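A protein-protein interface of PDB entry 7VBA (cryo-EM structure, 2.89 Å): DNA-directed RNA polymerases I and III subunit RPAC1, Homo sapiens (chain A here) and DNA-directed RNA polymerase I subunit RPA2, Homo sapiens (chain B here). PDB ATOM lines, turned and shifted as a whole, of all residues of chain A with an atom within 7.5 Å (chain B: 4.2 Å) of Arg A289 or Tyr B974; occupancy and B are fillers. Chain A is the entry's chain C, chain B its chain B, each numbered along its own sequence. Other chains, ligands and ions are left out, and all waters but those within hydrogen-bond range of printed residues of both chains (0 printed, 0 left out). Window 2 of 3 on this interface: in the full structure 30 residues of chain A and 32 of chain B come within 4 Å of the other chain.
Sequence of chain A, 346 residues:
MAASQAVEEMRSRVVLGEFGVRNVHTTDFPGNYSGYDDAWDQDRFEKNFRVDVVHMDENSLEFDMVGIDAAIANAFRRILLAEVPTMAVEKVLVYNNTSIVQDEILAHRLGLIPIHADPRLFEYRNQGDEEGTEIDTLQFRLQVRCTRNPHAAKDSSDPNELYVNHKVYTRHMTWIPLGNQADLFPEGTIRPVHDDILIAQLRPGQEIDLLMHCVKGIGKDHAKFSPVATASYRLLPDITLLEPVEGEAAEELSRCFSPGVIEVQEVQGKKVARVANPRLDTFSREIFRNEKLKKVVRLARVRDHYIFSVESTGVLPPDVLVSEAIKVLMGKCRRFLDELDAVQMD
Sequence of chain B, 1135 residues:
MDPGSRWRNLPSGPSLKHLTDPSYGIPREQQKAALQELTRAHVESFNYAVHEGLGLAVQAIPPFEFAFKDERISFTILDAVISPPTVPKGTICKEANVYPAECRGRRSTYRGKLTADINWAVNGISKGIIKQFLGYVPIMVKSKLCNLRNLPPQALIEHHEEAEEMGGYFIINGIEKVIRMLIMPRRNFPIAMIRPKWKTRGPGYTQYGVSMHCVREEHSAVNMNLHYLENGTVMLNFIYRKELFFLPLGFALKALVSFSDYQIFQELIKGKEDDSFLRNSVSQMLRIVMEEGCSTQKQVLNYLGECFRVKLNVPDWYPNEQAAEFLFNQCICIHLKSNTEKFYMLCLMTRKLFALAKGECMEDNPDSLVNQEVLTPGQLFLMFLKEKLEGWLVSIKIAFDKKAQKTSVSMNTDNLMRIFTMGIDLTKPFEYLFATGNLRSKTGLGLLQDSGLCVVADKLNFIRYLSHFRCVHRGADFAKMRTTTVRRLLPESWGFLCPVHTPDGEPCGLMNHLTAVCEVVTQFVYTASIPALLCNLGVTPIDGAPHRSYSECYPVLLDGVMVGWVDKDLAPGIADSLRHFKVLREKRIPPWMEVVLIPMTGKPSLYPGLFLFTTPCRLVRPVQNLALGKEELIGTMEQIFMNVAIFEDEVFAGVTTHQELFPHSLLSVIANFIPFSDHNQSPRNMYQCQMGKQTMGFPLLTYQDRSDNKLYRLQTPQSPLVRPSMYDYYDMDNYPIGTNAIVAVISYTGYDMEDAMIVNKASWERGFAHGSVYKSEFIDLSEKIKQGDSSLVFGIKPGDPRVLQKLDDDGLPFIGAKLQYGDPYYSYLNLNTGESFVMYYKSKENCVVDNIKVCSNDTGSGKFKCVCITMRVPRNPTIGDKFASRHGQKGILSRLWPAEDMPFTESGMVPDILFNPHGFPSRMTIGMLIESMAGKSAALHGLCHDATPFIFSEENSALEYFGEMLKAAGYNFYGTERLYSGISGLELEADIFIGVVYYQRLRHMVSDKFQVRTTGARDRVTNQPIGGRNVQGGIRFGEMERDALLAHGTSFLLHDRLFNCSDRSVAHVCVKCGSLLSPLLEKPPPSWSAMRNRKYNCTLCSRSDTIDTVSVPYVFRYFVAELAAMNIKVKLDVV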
ATOM      1  N   GLU A  18     -27.248  21.995  30.134  1.00  0.00           N
ATOM      2  CA  GLU A  18     -28.136  23.051  29.661  1.00  0.00           C
ATOM      3  C   GLU A  18     -29.300  23.276  30.619  1.00  0.00           C
ATOM      4  O   GLU A  18     -29.612  24.424  30.959  1.00  0.00           O
ATOM      5  CB  GLU A  18     -28.650  22.738  28.256  1.00  0.00           C
ATOM      6  CG  GLU A  18     -29.656  23.757  27.722  1.00  0.00           C
ATOM      7  CD  GLU A  18     -29.116  25.183  27.716  1.00  0.00           C
ATOM      8  OE1 GLU A  18     -28.035  25.422  28.293  1.00  0.00           O
ATOM      9  OE2 GLU A  18     -29.776  26.071  27.133  1.00  0.00           O
ATOM     10  N   CYS A 256     -20.225  27.292  17.130  1.00  0.00           N
ATOM     11  CA  CYS A 256     -21.084  27.272  18.307  1.00  0.00           C
ATOM     12  C   CYS A 256     -20.439  27.933  19.518  1.00  0.00           C
ATOM     13  O   CYS A 256     -21.025  27.916  20.605  1.00  0.00           O
ATOM     14  CB  CYS A 256     -21.478  25.833  18.644  1.00  0.00           C
ATOM     15  SG  CYS A 256     -22.308  24.954  17.302  1.00  0.00           S
ATOM     16  N   SER A 284     -22.938  31.003  25.909  1.00  0.00           N
ATOM     17  CA  SER A 284     -24.092  31.170  25.011  1.00  0.00           C
ATOM     18  C   SER A 284     -24.708  29.791  24.874  1.00  0.00           C
ATOM     19  O   SER A 284     -25.831  29.696  24.418  1.00  0.00           O
ATOM     20  CB  SER A 284     -23.619  31.660  23.717  1.00  0.00           C
ATOM     21  OG  SER A 284     -22.400  31.045  23.345  1.00  0.00           O
ATOM     22  N   ARG A 285     -23.976  28.754  25.244  1.00  0.00           N
ATOM     23  CA  ARG A 285     -24.549  27.413  25.282  1.00  0.00           C
ATOM     24  C   ARG A 285     -25.232  27.082  23.960  1.00  0.00           C
ATOM     25  O   ARG A 285     -26.316  26.501  23.924  1.00  0.00           O
ATOM     26  CB  ARG A 285     -25.529  27.259  26.446  1.00  0.00           C
ATOM     27  CG  ARG A 285     -24.873  27.127  27.809  1.00  0.00           C
ATOM     28  CD  ARG A 285     -24.672  28.491  28.436  1.00  0.00           C
ATOM     29  NE  ARG A 285     -25.957  29.109  28.750  1.00  0.00           N
ATOM     30  CZ  ARG A 285     -26.125  30.398  29.028  1.00  0.00           C
ATOM     31  NH1 ARG A 285     -25.088  31.221  29.026  1.00  0.00           N
ATOM     32  NH2 ARG A 285     -27.335  30.863  29.300  1.00  0.00           N
ATOM     33  N   GLU A 286     -24.590  27.458  22.857  1.00  0.00           N
ATOM     34  CA  GLU A 286     -25.131  27.165  21.538  1.00  0.00           C
ATOM     35  C   GLU A 286     -24.733  25.789  21.025  1.00  0.00           C
ATOM     36  O   GLU A 286     -25.303  25.329  20.031  1.00  0.00           O
ATOM     37  CB  GLU A 286     -24.698  28.230  20.529  1.00  0.00           C
ATOM     38  CG  GLU A 286     -25.321  29.586  20.780  1.00  0.00           C
ATOM     39  CD  GLU A 286     -26.822  29.566  20.601  1.00  0.00           C
ATOM     40  OE1 GLU A 286     -27.309  28.780  19.763  1.00  0.00           O
ATOM     41  OE2 GLU A 286     -27.518  30.330  21.300  1.00  0.00           O
ATOM     42  N   ILE A 287     -23.769  25.130  21.668  1.00  0.00           N
ATOM     43  CA  ILE A 287     -23.510  23.730  21.353  1.00  0.00           C
ATOM     44  C   ILE A 287     -24.695  22.871  21.764  1.00  0.00           C
ATOM     45  O   ILE A 287     -25.043  21.907  21.073  1.00  0.00           O
ATOM     46  CB  ILE A 287     -22.214  23.258  22.032  1.00  0.00           C
ATOM     47  CG1 ILE A 287     -22.123  23.831  23.443  1.00  0.00           C
ATOM     48  CG2 ILE A 287     -21.008  23.657  21.212  1.00  0.00           C
ATOM     49  CD1 ILE A 287     -21.057  23.191  24.287  1.00  0.00           C
ATOM     50  N   PHE A 288     -25.339  23.208  22.880  1.00  0.00           N
ATOM     51  CA  PHE A 288     -26.465  22.442  23.399  1.00  0.00           C
ATOM     52  C   PHE A 288     -27.653  22.410  22.452  1.00  0.00           C
ATOM     53  O   PHE A 288     -28.596  21.653  22.702  1.00  0.00           O
ATOM     54  CB  PHE A 288     -26.890  23.011  24.751  1.00  0.00           C
ATOM     55  CG  PHE A 288     -25.835  22.898  25.807  1.00  0.00           C
ATOM     56  CD1 PHE A 288     -24.792  22.002  25.663  1.00  0.00           C
ATOM     57  CD2 PHE A 288     -25.875  23.692  26.936  1.00  0.00           C
ATOM     58  CE1 PHE A 288     -23.814  21.893  26.630  1.00  0.00           C
ATOM     59  CE2 PHE A 288     -24.899  23.587  27.906  1.00  0.00           C
ATOM     60  CZ  PHE A 288     -23.868  22.685  27.752  1.00  0.00           C
ATOM     61  N   ARG A 289     -27.644  23.206  21.388  1.00  0.00           N
ATOM     62  CA  ARG A 289     -28.670  23.143  20.359  1.00  0.00           C
ATOM     63  C   ARG A 289     -28.267  22.248  19.200  1.00  0.00           C
ATOM     64  O   ARG A 289     -29.038  22.100  18.246  1.00  0.00           O
ATOM     65  CB  ARG A 289     -28.995  24.544  19.837  1.00  0.00           C
ATOM     66  CG  ARG A 289     -29.742  25.426  20.814  1.00  0.00           C
ATOM     67  CD  ARG A 289     -30.197  26.708  20.138  1.00  0.00           C
ATOM     68  NE  ARG A 289     -31.195  26.453  19.106  1.00  0.00           N
ATOM     69  CZ  ARG A 289     -31.015  26.702  17.815  1.00  0.00           C
ATOM     70  NH1 ARG A 289     -29.869  27.214  17.388  1.00  0.00           N
ATOM     71  NH2 ARG A 289     -31.980  26.437  16.945  1.00  0.00           N
ATOM     72  N   ASN A 290     -27.079  21.645  19.257  1.00  0.00           N
ATOM     73  CA  ASN A 290     -26.550  20.897  18.125  1.00  0.00           C
ATOM     74  C   ASN A 290     -27.020  19.450  18.084  1.00  0.00           C
ATOM     75  O   ASN A 290     -27.111  18.878  16.992  1.00  0.00           O
ATOM     76  CB  ASN A 290     -25.019  20.929  18.138  1.00  0.00           C
ATOM     77  CG  ASN A 290     -24.418  20.473  16.825  1.00  0.00           C
ATOM     78  OD1 ASN A 290     -25.136  20.150  15.880  1.00  0.00           O
ATOM     79  ND2 ASN A 290     -23.096  20.438  16.759  1.00  0.00           N
ATOM     80  N   GLU A 291     -27.322  18.847  19.232  1.00  0.00           N
ATOM     81  CA  GLU A 291     -27.919  17.520  19.351  1.00  0.00           C
ATOM     82  C   GLU A 291     -26.974  16.393  18.956  1.00  0.00           C
ATOM     83  O   GLU A 291     -27.351  15.222  19.078  1.00  0.00           O
ATOM     84  CB  GLU A 291     -29.206  17.392  18.522  1.00  0.00           C
ATOM     85  CG  GLU A 291     -30.134  18.583  18.653  1.00  0.00           C
ATOM     86  CD  GLU A 291     -31.317  18.509  17.713  1.00  0.00           C
ATOM     87  OE1 GLU A 291     -31.550  19.485  16.973  1.00  0.00           O
ATOM     88  OE2 GLU A 291     -32.012  17.473  17.710  1.00  0.00           O
ATOM     89  N   LYS A 292     -25.766  16.693  18.488  1.00  0.00           N
ATOM     90  CA  LYS A 292     -24.808  15.646  18.162  1.00  0.00           C
ATOM     91  C   LYS A 292     -23.447  15.979  18.751  1.00  0.00           C
ATOM     92  O   LYS A 292     -22.609  15.090  18.941  1.00  0.00           O
ATOM     93  CB  LYS A 292     -24.701  15.458  16.648  1.00  0.00           C
ATOM     94  CG  LYS A 292     -23.820  16.488  15.964  1.00  0.00           C
ATOM     95  CD  LYS A 292     -24.058  16.519  14.465  1.00  0.00           C
ATOM     96  CE  LYS A 292     -23.134  17.516  13.786  1.00  0.00           C
ATOM     97  NZ  LYS A 292     -21.704  17.127  13.926  1.00  0.00           N
ATOM     98  N   LEU A 293     -23.215  17.257  19.034  1.00  0.00           N
ATOM     99  CA  LEU A 293     -21.969  17.708  19.634  1.00  0.00           C
ATOM    100  C   LEU A 293     -22.138  18.179  21.070  1.00  0.00           C
ATOM    101  O   LEU A 293     -21.147  18.558  21.701  1.00  0.00           O
ATOM    102  CB  LEU A 293     -21.342  18.820  18.789  1.00  0.00           C
ATOM    103  CG  LEU A 293     -20.895  18.391  17.391  1.00  0.00           C
ATOM    104  CD1 LEU A 293     -20.277  19.555  16.644  1.00  0.00           C
ATOM    105  CD2 LEU A 293     -19.918  17.231  17.473  1.00  0.00           C
ATOM    106  N   LYS A 294     -23.360  18.176  21.603  1.00  0.00           N
ATOM    107  CA  LYS A 294     -23.520  18.412  23.032  1.00  0.00           C
ATOM    108  C   LYS A 294     -22.917  17.281  23.852  1.00  0.00           C
ATOM    109  O   LYS A 294     -22.677  17.457  25.050  1.00  0.00           O
ATOM    110  CB  LYS A 294     -24.995  18.586  23.391  1.00  0.00           C
ATOM    111  CG  LYS A 294     -25.884  17.424  22.988  1.00  0.00           C
ATOM    112  CD  LYS A 294     -27.338  17.700  23.335  1.00  0.00           C
ATOM    113  CE  LYS A 294     -28.002  18.595  22.303  1.00  0.00           C
ATOM    114  NZ  LYS A 294     -29.336  19.074  22.766  1.00  0.00           N
ATOM    115  N   MET B 933     -36.646  40.055  23.902  1.00  0.00           N
ATOM    116  CA  MET B 933     -35.662  39.563  22.945  1.00  0.00           C
ATOM    117  C   MET B 933     -35.532  40.497  21.750  1.00  0.00           C
ATOM    118  O   MET B 933     -34.420  40.747  21.271  1.00  0.00           O
ATOM    119  CB  MET B 933     -36.034  38.157  22.485  1.00  0.00           C
ATOM    120  CG  MET B 933     -36.264  37.173  23.607  1.00  0.00           C
ATOM    121  SD  MET B 933     -36.843  35.590  22.987  1.00  0.00           S
ATOM    122  CE  MET B 933     -35.405  35.044  22.079  1.00  0.00           C
ATOM    123  N   ASN B 972     -27.320  33.852  23.306  1.00  0.00           N
ATOM    124  CA  ASN B 972     -27.884  32.529  23.099  1.00  0.00           C
ATOM    125  C   ASN B 972     -29.299  32.628  22.550  1.00  0.00           C
ATOM    126  O   ASN B 972     -30.003  33.615  22.778  1.00  0.00           O
ATOM    127  CB  ASN B 972     -27.876  31.708  24.391  1.00  0.00           C
ATOM    128  CG  ASN B 972     -28.990  32.078  25.320  1.00  0.00           C
ATOM    129  OD1 ASN B 972     -29.365  33.244  25.419  1.00  0.00           O
ATOM    130  ND2 ASN B 972     -29.537  31.087  26.010  1.00  0.00           N
ATOM    131  N   PHE B 973     -29.696  31.588  21.816  1.00  0.00           N
ATOM    132  CA  PHE B 973     -30.989  31.571  21.149  1.00  0.00           C
ATOM    133  C   PHE B 973     -32.109  31.986  22.092  1.00  0.00           C
ATOM    134  O   PHE B 973     -32.828  32.956  21.830  1.00  0.00           O
ATOM    135  CB  PHE B 973     -31.254  30.171  20.600  1.00  0.00           C
ATOM    136  CG  PHE B 973     -32.432  30.086  19.679  1.00  0.00           C
ATOM    137  CD1 PHE B 973     -32.286  30.320  18.326  1.00  0.00           C
ATOM    138  CD2 PHE B 973     -33.691  29.799  20.170  1.00  0.00           C
ATOM    139  CE1 PHE B 973     -33.364  30.237  17.480  1.00  0.00           C
ATOM    140  CE2 PHE B 973     -34.774  29.724  19.327  1.00  0.00           C
ATOM    141  CZ  PHE B 973     -34.609  29.943  17.980  1.00  0.00           C
ATOM    142  N   TYR B 974     -32.261  31.269  23.204  1.00  0.00           N
ATOM    143  CA  TYR B 974     -33.452  31.400  24.034  1.00  0.00           C
ATOM    144  C   TYR B 974     -33.462  32.670  24.870  1.00  0.00           C
ATOM    145  O   TYR B 974     -34.375  32.852  25.679  1.00  0.00           O
ATOM    146  CB  TYR B 974     -33.583  30.171  24.928  1.00  0.00           C
ATOM    147  CG  TYR B 974     -33.519  28.890  24.136  1.00  0.00           C
ATOM    148  CD1 TYR B 974     -34.531  28.546  23.257  1.00  0.00           C
ATOM    149  CD2 TYR B 974     -32.436  28.035  24.252  1.00  0.00           C
ATOM    150  CE1 TYR B 974     -34.472  27.386  22.523  1.00  0.00           C
ATOM    151  CE2 TYR B 974     -32.368  26.872  23.523  1.00  0.00           C
ATOM    152  CZ  TYR B 974     -33.388  26.552  22.660  1.00  0.00           C
ATOM    153  OH  TYR B 974     -33.327  25.389  21.930  1.00  0.00           O
ATOM    154  N   GLY B 975     -32.473  33.542  24.712  1.00  0.00           N
ATOM    155  CA  GLY B 975     -32.508  34.831  25.362  1.00  0.00           C
ATOM    156  C   GLY B 975     -32.082  34.839  26.809  1.00  0.00           C
ATOM    157  O   GLY B 975     -32.270  35.856  27.484  1.00  0.00           O
ATOM    158  N   THR B 976     -31.522  33.744  27.310  1.00  0.00           N
ATOM    159  CA  THR B 976     -31.095  33.636  28.698  1.00  0.00           C
ATOM    160  C   THR B 976     -29.592  33.856  28.770  1.00  0.00           C
ATOM    161  O   THR B 976     -28.826  33.162  28.095  1.00  0.00           O
ATOM    162  CB  THR B 976     -31.452  32.270  29.285  1.00  0.00           C
ATOM    163  OG1 THR B 976     -30.618  31.267  28.700  1.00  0.00           O
ATOM    164  CG2 THR B 976     -32.906  31.930  29.017  1.00  0.00           C
ATOM    165  N   PHE B 993     -33.450  35.091  32.224  1.00  0.00           N
ATOM    166  CA  PHE B 993     -33.961  35.676  30.993  1.00  0.00           C
ATOM    167  C   PHE B 993     -33.926  37.192  31.120  1.00  0.00           C
ATOM    168  O   PHE B 993     -34.713  37.772  31.871  1.00  0.00           O
ATOM    169  CB  PHE B 993     -35.380  35.180  30.729  1.00  0.00           C
ATOM    170  CG  PHE B 993     -36.017  35.770  29.510  1.00  0.00           C
ATOM    171  CD1 PHE B 993     -35.887  35.157  28.281  1.00  0.00           C
ATOM    172  CD2 PHE B 993     -36.766  36.926  29.596  1.00  0.00           C
ATOM    173  CE1 PHE B 993     -36.477  35.693  27.163  1.00  0.00           C
ATOM    174  CE2 PHE B 993     -37.358  37.464  28.479  1.00  0.00           C
ATOM    175  CZ  PHE B 993     -37.211  36.845  27.262  1.00  0.00           C
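Among the printed residues, pairs that only touch across the chains: Glu A286 with Asn B972 (2.9 Å), Ser A284 with Asn B972 (2.9 Å), Arg A289 with Phe B973 (3.7 Å), Arg A289 with Tyr B974 (3.7 Å) and Arg A285 with Asn B972 (3.97 Å).
The backbone carbonyl oxygen of Thr B976 is in hydrogen-bond range of the guanidinium group of Arg A285, 3.0 Å away.
OE2 of Glu A286 sits at hydrogen-bond distance from N of Phe B973, at 2.6 Å.
Of the 13 printed residues of chain A, 4 touch a printed residue of chain B.
Among the printed residues, 7 pairs touch across the chains.
OD1 of Asn B972 sits at hydrogen-bond distance from N of Gly B975 (3.2 Å).
OE1 of Glu A286 is in salt-bridge range of NH1 of Arg A289 (3.8 Å).
The backbone carbonyl oxygen of Thr B976 lies close to the side-chain amide oxygen of Asn B972.
Of the printed residues of chain B, Arg A289 touches Phe B973 and Tyr B974.
Of the printed residues of chain A, Phe B973 touches Glu A286 (2.6 Å) and Arg A289 (3.7 Å).
Of the printed residues of chain A, Asn B972 touches Ser A284 (2.9 Å), Arg A285 (3.97 Å) and Glu A286 (2.9 Å).
Of the printed residues of chain B, Arg A285 touches Asn B972 (3.97 Å) and Thr B976 (3.0 Å).
Printed residues of chain B within 4 Å of Ser A284: Asn B972.
Asn A290 touches none of the printed residues of chain B.
The nearest printed residue of chain B that does not touch Arg A289 is Asn B972 (6.5 Å).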
